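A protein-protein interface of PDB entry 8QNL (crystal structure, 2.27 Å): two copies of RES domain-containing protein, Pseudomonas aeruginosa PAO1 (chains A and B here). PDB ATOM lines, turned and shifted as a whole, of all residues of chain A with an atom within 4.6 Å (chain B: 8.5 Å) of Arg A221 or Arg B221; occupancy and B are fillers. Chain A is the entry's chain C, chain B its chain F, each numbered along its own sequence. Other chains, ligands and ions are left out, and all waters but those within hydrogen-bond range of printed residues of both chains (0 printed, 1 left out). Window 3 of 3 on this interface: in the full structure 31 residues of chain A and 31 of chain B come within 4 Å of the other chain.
Arg A221 touches just one residue of chain B: Arg B221. Of chain A, only Arg A219 (2.8 Å), Arg A221 (3.3 Å) and Asn A222 (2.9 Å) come within 4 Å of Arg B221. Printed residues of chain B within 4 Å of Asn A222: Arg B221 (2.9 Å). Of the printed residues of chain A, Leu B223 touches Leu A223. Of the printed residues of chain B, Arg A219 touches Arg B221 and Asn B222. Of the printed residues of chain A, Asn B222 touches Arg A219 (3.1 Å). The nearest printed residue of chain A that does not touch Arg B221 is Pro A220 (4.7 Å).
Among the printed residues, pairs that only touch across the chains: Arg A221 with Arg B221 and Leu A223 with Leu B223.
Printed residues of chain B that touch a printed residue of chain A: Arg B221, Asn B222 and Leu B223. Hydrophobic or aromatic side chains of chain B within 4 Å of the printed part of chain A: Leu B223. Printed residues of chain A that touch a printed residue of chain B: Arg A219, Arg A221, Asn A222 and Leu A223. Hydrophobic or aromatic side chains of chain A within 4 Å of the printed part of chain B: Leu A223.
The backbone NH (N) of Glu A146 lies within hydrogen-bond range of the backbone carbonyl oxygen (O) of Arg A221 (2.6 Å). The side-chain hydroxyl (OG1) of Thr B224 sits at hydrogen-bond distance from the backbone carbonyl oxygen (O) of Asn B222 (3.1 Å). N of Glu B146 lies within hydrogen-bond range of O of Arg B221, at 2.6 Å. The guanidinium group (NH1) of Arg A221 is in salt-bridge range of the side-chain carboxylate (OE2) of Glu A217 (2.9 Å). OE2 of Glu A146 is in hydrogen-bond range of ND2 of Asn A222, at 2.7 Å. The side-chain amide nitrogen (ND2) of Asn B222 sits at hydrogen-bond distance from the side-chain carboxylate (OE2) of Glu B146 (2.9 Å).
Arg A219 touches Asn B222, but with the chains exchanged Asn A222 does not touch Arg B219 (6.6 Å). Arg A221 touches its own counterpart, Arg B221. Asn A222 touches Arg B221, but with the chains exchanged Arg A221 does not touch Asn B222 (7.0 Å). Leu A223 touches its own counterpart, Leu B223. 9 positions are printed for both chains. Of the 5 pairs that touch across the chains among the printed residues, 2 have their exchanged pair printed and touching as well.
The backbone NH (N) of Asn A222 sits close to the guanidinium group (NH2) of Arg B221, 2.9 Å away. OD1 of Asn B222 sits at hydrogen-bond distance from NH2 of Arg A219, 3.1 Å away. NH2 of Arg A219 sits close to NH2 of Arg B221, 2.8 Å away.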
ATOM      1  N   ARG A  33      -6.697 -30.537   3.034  1.00  0.00           N
ATOM      2  CA  ARG A  33      -6.869 -30.092   4.408  1.00  0.00           C
ATOM      3  C   ARG A  33      -6.169 -31.064   5.349  1.00  0.00           C
ATOM      4  O   ARG A  33      -5.899 -32.216   4.999  1.00  0.00           O
ATOM      5  CB  ARG A  33      -8.355 -29.984   4.779  1.00  0.00           C
ATOM      6  CG  ARG A  33      -9.191 -29.154   3.812  1.00  0.00           C
ATOM      7  CD  ARG A  33      -8.930 -27.658   3.954  1.00  0.00           C
ATOM      8  NE  ARG A  33      -9.491 -27.118   5.190  1.00  0.00           N
ATOM      9  CZ  ARG A  33      -9.601 -25.822   5.460  1.00  0.00           C
ATOM     10  NH1 ARG A  33      -9.195 -24.919   4.578  1.00  0.00           N
ATOM     11  NH2 ARG A  33     -10.121 -25.426   6.614  1.00  0.00           N
ATOM     12  N   PHE A 145      -7.578 -29.030  15.583  1.00  0.00           N
ATOM     13  CA  PHE A 145      -7.828 -27.934  14.660  1.00  0.00           C
ATOM     14  C   PHE A 145      -7.585 -28.404  13.232  1.00  0.00           C
ATOM     15  O   PHE A 145      -6.922 -29.417  12.989  1.00  0.00           O
ATOM     16  CB  PHE A 145      -6.970 -26.700  14.984  1.00  0.00           C
ATOM     17  CG  PHE A 145      -5.489 -26.908  14.796  1.00  0.00           C
ATOM     18  CD1 PHE A 145      -4.886 -26.638  13.578  1.00  0.00           C
ATOM     19  CD2 PHE A 145      -4.697 -27.339  15.848  1.00  0.00           C
ATOM     20  CE1 PHE A 145      -3.530 -26.816  13.404  1.00  0.00           C
ATOM     21  CE2 PHE A 145      -3.338 -27.517  15.681  1.00  0.00           C
ATOM     22  CZ  PHE A 145      -2.754 -27.257  14.456  1.00  0.00           C
ATOM     23  N   GLU A 146      -8.143 -27.654  12.286  1.00  0.00           N
ATOM     24  CA  GLU A 146      -8.014 -27.934  10.866  1.00  0.00           C
ATOM     25  C   GLU A 146      -7.352 -26.753  10.167  1.00  0.00           C
ATOM     26  O   GLU A 146      -7.399 -25.616  10.645  1.00  0.00           O
ATOM     27  CB  GLU A 146      -9.379 -28.226  10.237  1.00  0.00           C
ATOM     28  CG  GLU A 146     -10.127 -29.352  10.924  1.00  0.00           C
ATOM     29  CD  GLU A 146     -11.602 -29.358  10.589  1.00  0.00           C
ATOM     30  OE1 GLU A 146     -12.016 -28.562   9.720  1.00  0.00           O
ATOM     31  OE2 GLU A 146     -12.346 -30.153  11.201  1.00  0.00           O
ATOM     32  N   GLU A 217      -4.200 -20.677   4.801  1.00  0.00           N
ATOM     33  CA  GLU A 217      -4.947 -19.753   5.634  1.00  0.00           C
ATOM     34  C   GLU A 217      -4.045 -19.115   6.688  1.00  0.00           C
ATOM     35  O   GLU A 217      -2.892 -19.504   6.888  1.00  0.00           O
ATOM     36  CB  GLU A 217      -6.126 -20.465   6.298  1.00  0.00           C
ATOM     37  CG  GLU A 217      -7.149 -21.026   5.313  1.00  0.00           C
ATOM     38  CD  GLU A 217      -8.070 -22.067   5.936  1.00  0.00           C
ATOM     39  OE1 GLU A 217      -7.667 -22.714   6.927  1.00  0.00           O
ATOM     40  OE2 GLU A 217      -9.199 -22.239   5.429  1.00  0.00           O
ATOM     41  N   ARG A 219      -5.259 -18.613   9.998  1.00  0.00           N
ATOM     42  CA  ARG A 219      -5.715 -18.995  11.317  1.00  0.00           C
ATOM     43  C   ARG A 219      -6.241 -20.424  11.282  1.00  0.00           C
ATOM     44  O   ARG A 219      -6.985 -20.788  10.359  1.00  0.00           O
ATOM     45  CB  ARG A 219      -6.813 -18.036  11.803  1.00  0.00           C
ATOM     46  CG  ARG A 219      -7.744 -18.615  12.848  1.00  0.00           C
ATOM     47  CD  ARG A 219      -9.121 -17.977  12.762  1.00  0.00           C
ATOM     48  NE  ARG A 219     -10.153 -18.864  13.288  1.00  0.00           N
ATOM     49  CZ  ARG A 219     -11.384 -18.944  12.798  1.00  0.00           C
ATOM     50  NH1 ARG A 219     -11.738 -18.198  11.763  1.00  0.00           N
ATOM     51  NH2 ARG A 219     -12.257 -19.780  13.336  1.00  0.00           N
ATOM     52  N   PRO A 220      -5.865 -21.254  12.257  1.00  0.00           N
ATOM     53  CA  PRO A 220      -6.398 -22.622  12.307  1.00  0.00           C
ATOM     54  C   PRO A 220      -7.907 -22.618  12.513  1.00  0.00           C
ATOM     55  O   PRO A 220      -8.460 -21.755  13.196  1.00  0.00           O
ATOM     56  CB  PRO A 220      -5.668 -23.244  13.502  1.00  0.00           C
ATOM     57  CG  PRO A 220      -5.241 -22.073  14.337  1.00  0.00           C
ATOM     58  CD  PRO A 220      -4.936 -20.979  13.363  1.00  0.00           C
ATOM     59  N   ARG A 221      -8.573 -23.608  11.921  1.00  0.00           N
ATOM     60  CA  ARG A 221     -10.027 -23.636  11.856  1.00  0.00           C
ATOM     61  C   ARG A 221     -10.590 -24.802  12.661  1.00  0.00           C
ATOM     62  O   ARG A 221      -9.930 -25.828  12.853  1.00  0.00           O
ATOM     63  CB  ARG A 221     -10.500 -23.723  10.394  1.00  0.00           C
ATOM     64  CG  ARG A 221     -10.036 -22.546   9.535  1.00  0.00           C
ATOM     65  CD  ARG A 221     -11.131 -21.500   9.364  1.00  0.00           C
ATOM     66  NE  ARG A 221     -12.049 -21.868   8.290  1.00  0.00           N
ATOM     67  CZ  ARG A 221     -11.991 -21.380   7.054  1.00  0.00           C
ATOM     68  NH1 ARG A 221     -11.063 -20.488   6.731  1.00  0.00           N
ATOM     69  NH2 ARG A 221     -12.867 -21.780   6.140  1.00  0.00           N
ATOM     70  N   ASN A 222     -11.822 -24.622  13.138  1.00  0.00           N
ATOM     71  CA  ASN A 222     -12.576 -25.663  13.839  1.00  0.00           C
ATOM     72  C   ASN A 222     -11.834 -26.157  15.084  1.00  0.00           C
ATOM     73  O   ASN A 222     -11.710 -27.361  15.327  1.00  0.00           O
ATOM     74  CB  ASN A 222     -12.906 -26.825  12.901  1.00  0.00           C
ATOM     75  CG  ASN A 222     -14.000 -27.713  13.447  1.00  0.00           C
ATOM     76  OD1 ASN A 222     -14.761 -27.303  14.326  1.00  0.00           O
ATOM     77  ND2 ASN A 222     -14.091 -28.934  12.933  1.00  0.00           N
ATOM     78  N   LEU A 223     -11.329 -25.212  15.874  1.00  0.00           N
ATOM     79  CA  LEU A 223     -10.696 -25.560  17.139  1.00  0.00           C
ATOM     80  C   LEU A 223     -11.716 -26.249  18.039  1.00  0.00           C
ATOM     81  O   LEU A 223     -12.749 -25.663  18.379  1.00  0.00           O
ATOM     82  CB  LEU A 223     -10.135 -24.306  17.806  1.00  0.00           C
ATOM     83  CG  LEU A 223      -9.194 -24.525  18.993  1.00  0.00           C
ATOM     84  CD1 LEU A 223      -7.978 -25.331  18.570  1.00  0.00           C
ATOM     85  CD2 LEU A 223      -8.771 -23.189  19.585  1.00  0.00           C
ATOM     86  N   ARG B  33     -23.313 -10.151  12.943  1.00  0.00           N
ATOM     87  CA  ARG B  33     -22.582 -11.187  13.658  1.00  0.00           C
ATOM     88  C   ARG B  33     -22.749 -10.989  15.158  1.00  0.00           C
ATOM     89  O   ARG B  33     -23.066  -9.895  15.633  1.00  0.00           O
ATOM     90  CB  ARG B  33     -21.096 -11.166  13.287  1.00  0.00           C
ATOM     91  CG  ARG B  33     -20.826 -11.338  11.801  1.00  0.00           C
ATOM     92  CD  ARG B  33     -20.818 -12.803  11.404  1.00  0.00           C
ATOM     93  NE  ARG B  33     -19.624 -13.490  11.890  1.00  0.00           N
ATOM     94  CZ  ARG B  33     -19.357 -14.774  11.669  1.00  0.00           C
ATOM     95  NH1 ARG B  33     -20.203 -15.516  10.966  1.00  0.00           N
ATOM     96  NH2 ARG B  33     -18.245 -15.315  12.151  1.00  0.00           N
ATOM     97  N   LEU B  34     -22.535 -12.067  15.906  1.00  0.00           N
ATOM     98  CA  LEU B  34     -22.582 -12.004  17.358  1.00  0.00           C
ATOM     99  C   LEU B  34     -21.427 -12.812  17.928  1.00  0.00           C
ATOM    100  O   LEU B  34     -20.949 -13.765  17.309  1.00  0.00           O
ATOM    101  CB  LEU B  34     -23.921 -12.513  17.916  1.00  0.00           C
ATOM    102  CG  LEU B  34     -24.370 -13.948  17.616  1.00  0.00           C
ATOM    103  CD1 LEU B  34     -23.808 -14.944  18.623  1.00  0.00           C
ATOM    104  CD2 LEU B  34     -25.886 -14.019  17.589  1.00  0.00           C
ATOM    105  N   VAL B  35     -20.982 -12.414  19.112  1.00  0.00           N
ATOM    106  CA  VAL B  35     -19.932 -13.113  19.837  1.00  0.00           C
ATOM    107  C   VAL B  35     -20.420 -13.315  21.262  1.00  0.00           C
ATOM    108  O   VAL B  35     -21.102 -12.452  21.824  1.00  0.00           O
ATOM    109  CB  VAL B  35     -18.599 -12.337  19.794  1.00  0.00           C
ATOM    110  CG1 VAL B  35     -18.829 -10.902  20.175  1.00  0.00           C
ATOM    111  CG2 VAL B  35     -17.558 -12.980  20.700  1.00  0.00           C
ATOM    112  N   ARG B  36     -20.091 -14.466  21.839  1.00  0.00           N
ATOM    113  CA  ARG B  36     -20.694 -14.870  23.097  1.00  0.00           C
ATOM    114  C   ARG B  36     -19.675 -15.655  23.903  1.00  0.00           C
ATOM    115  O   ARG B  36     -18.978 -16.511  23.352  1.00  0.00           O
ATOM    116  CB  ARG B  36     -21.945 -15.706  22.826  1.00  0.00           C
ATOM    117  CG  ARG B  36     -22.678 -16.166  24.047  1.00  0.00           C
ATOM    118  CD  ARG B  36     -23.947 -16.857  23.618  1.00  0.00           C
ATOM    119  NE  ARG B  36     -24.316 -17.915  24.543  1.00  0.00           N
ATOM    120  CZ  ARG B  36     -25.195 -17.771  25.526  1.00  0.00           C
ATOM    121  NH1 ARG B  36     -25.804 -16.609  25.715  1.00  0.00           N
ATOM    122  NH2 ARG B  36     -25.460 -18.794  26.319  1.00  0.00           N
ATOM    123  N   HIS B  78     -26.894 -26.543  16.870  1.00  0.00           N
ATOM    124  CA  HIS B  78     -25.745 -26.977  17.646  1.00  0.00           C
ATOM    125  C   HIS B  78     -26.023 -26.811  19.139  1.00  0.00           C
ATOM    126  O   HIS B  78     -26.854 -26.000  19.557  1.00  0.00           O
ATOM    127  CB  HIS B  78     -24.509 -26.176  17.236  1.00  0.00           C
ATOM    128  CG  HIS B  78     -23.232 -26.661  17.850  1.00  0.00           C
ATOM    129  ND1 HIS B  78     -22.752 -26.180  19.050  1.00  0.00           N
ATOM    130  CD2 HIS B  78     -22.323 -27.567  17.418  1.00  0.00           C
ATOM    131  CE1 HIS B  78     -21.609 -26.776  19.334  1.00  0.00           C
ATOM    132  NE2 HIS B  78     -21.326 -27.623  18.361  1.00  0.00           N
ATOM    133  N   LEU B  80     -24.277 -25.424  21.471  1.00  0.00           N
ATOM    134  CA  LEU B  80     -24.025 -24.081  21.985  1.00  0.00           C
ATOM    135  C   LEU B  80     -25.076 -23.076  21.535  1.00  0.00           C
ATOM    136  O   LEU B  80     -25.223 -22.027  22.172  1.00  0.00           O
ATOM    137  CB  LEU B  80     -22.637 -23.600  21.560  1.00  0.00           C
ATOM    138  CG  LEU B  80     -21.463 -24.403  22.116  1.00  0.00           C
ATOM    139  CD1 LEU B  80     -20.148 -23.904  21.541  1.00  0.00           C
ATOM    140  CD2 LEU B  80     -21.450 -24.329  23.636  1.00  0.00           C
ATOM    141  N   LEU B  81     -25.804 -23.367  20.459  1.00  0.00           N
ATOM    142  CA  LEU B  81     -26.827 -22.451  19.975  1.00  0.00           C
ATOM    143  C   LEU B  81     -28.201 -22.738  20.565  1.00  0.00           C
ATOM    144  O   LEU B  81     -28.989 -21.806  20.747  1.00  0.00           O
ATOM    145  CB  LEU B  81     -26.904 -22.510  18.446  1.00  0.00           C
ATOM    146  CG  LEU B  81     -25.646 -22.102  17.676  1.00  0.00           C
ATOM    147  CD1 LEU B  81     -25.920 -22.080  16.180  1.00  0.00           C
ATOM    148  CD2 LEU B  81     -25.139 -20.750  18.149  1.00  0.00           C
ATOM    149  N   SER B 144     -15.300 -18.632  23.939  1.00  0.00           N
ATOM    150  CA  SER B 144     -16.067 -17.710  23.118  1.00  0.00           C
ATOM    151  C   SER B 144     -16.295 -18.316  21.739  1.00  0.00           C
ATOM    152  O   SER B 144     -15.463 -19.073  21.232  1.00  0.00           O
ATOM    153  CB  SER B 144     -15.359 -16.357  22.978  1.00  0.00           C
ATOM    154  OG  SER B 144     -14.257 -16.435  22.089  1.00  0.00           O
ATOM    155  N   PHE B 145     -17.436 -17.981  21.140  1.00  0.00           N
ATOM    156  CA  PHE B 145     -17.745 -18.403  19.782  1.00  0.00           C
ATOM    157  C   PHE B 145     -18.511 -17.296  19.073  1.00  0.00           C
ATOM    158  O   PHE B 145     -19.108 -16.417  19.702  1.00  0.00           O
ATOM    159  CB  PHE B 145     -18.545 -19.716  19.748  1.00  0.00           C
ATOM    160  CG  PHE B 145     -19.909 -19.632  20.388  1.00  0.00           C
ATOM    161  CD1 PHE B 145     -21.033 -19.326  19.633  1.00  0.00           C
ATOM    162  CD2 PHE B 145     -20.070 -19.889  21.740  1.00  0.00           C
ATOM    163  CE1 PHE B 145     -22.285 -19.261  20.219  1.00  0.00           C
ATOM    164  CE2 PHE B 145     -21.321 -19.824  22.332  1.00  0.00           C
ATOM    165  CZ  PHE B 145     -22.427 -19.509  21.570  1.00  0.00           C
ATOM    166  N   GLU B 146     -18.482 -17.349  17.745  1.00  0.00           N
ATOM    167  CA  GLU B 146     -19.164 -16.383  16.901  1.00  0.00           C
ATOM    168  C   GLU B 146     -20.250 -17.087  16.103  1.00  0.00           C
ATOM    169  O   GLU B 146     -20.201 -18.299  15.884  1.00  0.00           O
ATOM    170  CB  GLU B 146     -18.178 -15.679  15.960  1.00  0.00           C
ATOM    171  CG  GLU B 146     -17.012 -15.020  16.681  1.00  0.00           C
ATOM    172  CD  GLU B 146     -15.888 -14.624  15.741  1.00  0.00           C
ATOM    173  OE1 GLU B 146     -16.077 -14.716  14.509  1.00  0.00           O
ATOM    174  OE2 GLU B 146     -14.812 -14.228  16.236  1.00  0.00           O
ATOM    175  N   ALA B 147     -21.247 -16.314  15.679  1.00  0.00           N
ATOM    176  CA  ALA B 147     -22.341 -16.861  14.888  1.00  0.00           C
ATOM    177  C   ALA B 147     -22.949 -15.748  14.048  1.00  0.00           C
ATOM    178  O   ALA B 147     -22.991 -14.592  14.478  1.00  0.00           O
ATOM    179  CB  ALA B 147     -23.412 -17.502  15.776  1.00  0.00           C
ATOM    180  N   GLY B 148     -23.402 -16.099  12.848  1.00  0.00           N
ATOM    181  CA  GLY B 148     -24.124 -15.163  12.007  1.00  0.00           C
ATOM    182  C   GLY B 148     -25.617 -15.233  12.283  1.00  0.00           C
ATOM    183  O   GLY B 148     -26.187 -16.313  12.435  1.00  0.00           O
ATOM    184  N   GLU B 217     -26.430 -19.880  10.174  1.00  0.00           N
ATOM    185  CA  GLU B 217     -25.842 -21.209  10.148  1.00  0.00           C
ATOM    186  C   GLU B 217     -26.424 -22.055  11.278  1.00  0.00           C
ATOM    187  O   GLU B 217     -27.209 -21.586  12.107  1.00  0.00           O
ATOM    188  CB  GLU B 217     -24.320 -21.119  10.262  1.00  0.00           C
ATOM    189  CG  GLU B 217     -23.690 -20.029   9.417  1.00  0.00           C
ATOM    190  CD  GLU B 217     -22.254 -19.766   9.816  1.00  0.00           C
ATOM    191  OE1 GLU B 217     -21.696 -20.598  10.560  1.00  0.00           O
ATOM    192  OE2 GLU B 217     -21.687 -18.731   9.401  1.00  0.00           O
ATOM    193  N   LYS B 218     -26.021 -23.322  11.315  1.00  0.00           N
ATOM    194  CA  LYS B 218     -26.383 -24.216  12.404  1.00  0.00           C
ATOM    195  C   LYS B 218     -25.207 -24.502  13.327  1.00  0.00           C
ATOM    196  O   LYS B 218     -25.376 -25.211  14.322  1.00  0.00           O
ATOM    197  CB  LYS B 218     -26.944 -25.528  11.846  1.00  0.00           C
ATOM    198  CG  LYS B 218     -28.140 -25.335  10.929  1.00  0.00           C
ATOM    199  CD  LYS B 218     -28.262 -26.464   9.916  1.00  0.00           C
ATOM    200  CE  LYS B 218     -29.419 -26.218   8.959  1.00  0.00           C
ATOM    201  NZ  LYS B 218     -29.350 -24.865   8.337  1.00  0.00           N
ATOM    202  N   ARG B 219     -24.028 -23.956  13.028  1.00  0.00           N
ATOM    203  CA  ARG B 219     -22.811 -24.213  13.771  1.00  0.00           C
ATOM    204  C   ARG B 219     -22.202 -22.908  14.276  1.00  0.00           C
ATOM    205  O   ARG B 219     -22.292 -21.871  13.607  1.00  0.00           O
ATOM    206  CB  ARG B 219     -21.773 -24.949  12.907  1.00  0.00           C
ATOM    207  CG  ARG B 219     -21.355 -24.193  11.643  1.00  0.00           C
ATOM    208  CD  ARG B 219     -19.871 -24.383  11.322  1.00  0.00           C
ATOM    209  NE  ARG B 219     -19.416 -23.521  10.230  1.00  0.00           N
ATOM    210  CZ  ARG B 219     -19.135 -22.226  10.365  1.00  0.00           C
ATOM    211  NH1 ARG B 219     -19.274 -21.636  11.545  1.00  0.00           N
ATOM    212  NH2 ARG B 219     -18.723 -21.517   9.320  1.00  0.00           N
ATOM    213  N   PRO B 220     -21.591 -22.927  15.453  1.00  0.00           N
ATOM    214  CA  PRO B 220     -20.825 -21.767  15.911  1.00  0.00           C
ATOM    215  C   PRO B 220     -19.466 -21.713  15.231  1.00  0.00           C
ATOM    216  O   PRO B 220     -18.951 -22.710  14.724  1.00  0.00           O
ATOM    217  CB  PRO B 220     -20.682 -22.021  17.416  1.00  0.00           C
ATOM    218  CG  PRO B 220     -20.703 -23.506  17.535  1.00  0.00           C
ATOM    219  CD  PRO B 220     -21.638 -24.000  16.461  1.00  0.00           C
ATOM    220  N   ARG B 221     -18.891 -20.515  15.220  1.00  0.00           N
ATOM    221  CA  ARG B 221     -17.645 -20.266  14.518  1.00  0.00           C
ATOM    222  C   ARG B 221     -16.613 -19.677  15.471  1.00  0.00           C
ATOM    223  O   ARG B 221     -16.955 -18.964  16.418  1.00  0.00           O
ATOM    224  CB  ARG B 221     -17.860 -19.323  13.323  1.00  0.00           C
ATOM    225  CG  ARG B 221     -16.683 -19.254  12.365  1.00  0.00           C
ATOM    226  CD  ARG B 221     -16.280 -20.653  11.932  1.00  0.00           C
ATOM    227  NE  ARG B 221     -14.844 -20.878  12.018  1.00  0.00           N
ATOM    228  CZ  ARG B 221     -14.294 -22.083  12.038  1.00  0.00           C
ATOM    229  NH1 ARG B 221     -15.063 -23.156  11.991  1.00  0.00           N
ATOM    230  NH2 ARG B 221     -12.983 -22.215  12.112  1.00  0.00           N
ATOM    231  N   ASN B 222     -15.346 -20.009  15.215  1.00  0.00           N
ATOM    232  CA  ASN B 222     -14.203 -19.432  15.923  1.00  0.00           C
ATOM    233  C   ASN B 222     -14.267 -19.696  17.428  1.00  0.00           C
ATOM    234  O   ASN B 222     -14.111 -18.790  18.248  1.00  0.00           O
ATOM    235  CB  ASN B 222     -14.083 -17.934  15.637  1.00  0.00           C
ATOM    236  CG  ASN B 222     -12.695 -17.404  15.916  1.00  0.00           C
ATOM    237  OD1 ASN B 222     -11.726 -18.165  15.935  1.00  0.00           O
ATOM    238  ND2 ASN B 222     -12.586 -16.098  16.134  1.00  0.00           N
ATOM    239  N   LEU B 223     -14.479 -20.960  17.789  1.00  0.00           N
ATOM    240  CA  LEU B 223     -14.456 -21.356  19.192  1.00  0.00           C
ATOM    241  C   LEU B 223     -13.064 -21.122  19.775  1.00  0.00           C
ATOM    242  O   LEU B 223     -12.078 -21.687  19.292  1.00  0.00           O
ATOM    243  CB  LEU B 223     -14.865 -22.820  19.331  1.00  0.00           C
ATOM    244  CG  LEU B 223     -15.070 -23.360  20.748  1.00  0.00           C
ATOM    245  CD1 LEU B 223     -16.201 -22.623  21.438  1.00  0.00           C
ATOM    246  CD2 LEU B 223     -15.353 -24.853  20.701  1.00  0.00           C
ATOM    247  N   THR B 224     -12.989 -20.298  20.818  1.00  0.00           N
ATOM    248  CA  THR B 224     -11.720 -19.864  21.399  1.00  0.00           C
ATOM    249  C   THR B 224     -11.760 -20.085  22.905  1.00  0.00           C
ATOM    250  O   THR B 224     -12.681 -19.579  23.576  1.00  0.00           O
ATOM    251  CB  THR B 224     -11.461 -18.388  21.077  1.00  0.00           C
ATOM    252  OG1 THR B 224     -11.441 -18.201  19.656  1.00  0.00           O
ATOM    253  CG2 THR B 224     -10.136 -17.924  21.671  1.00  0.00           C
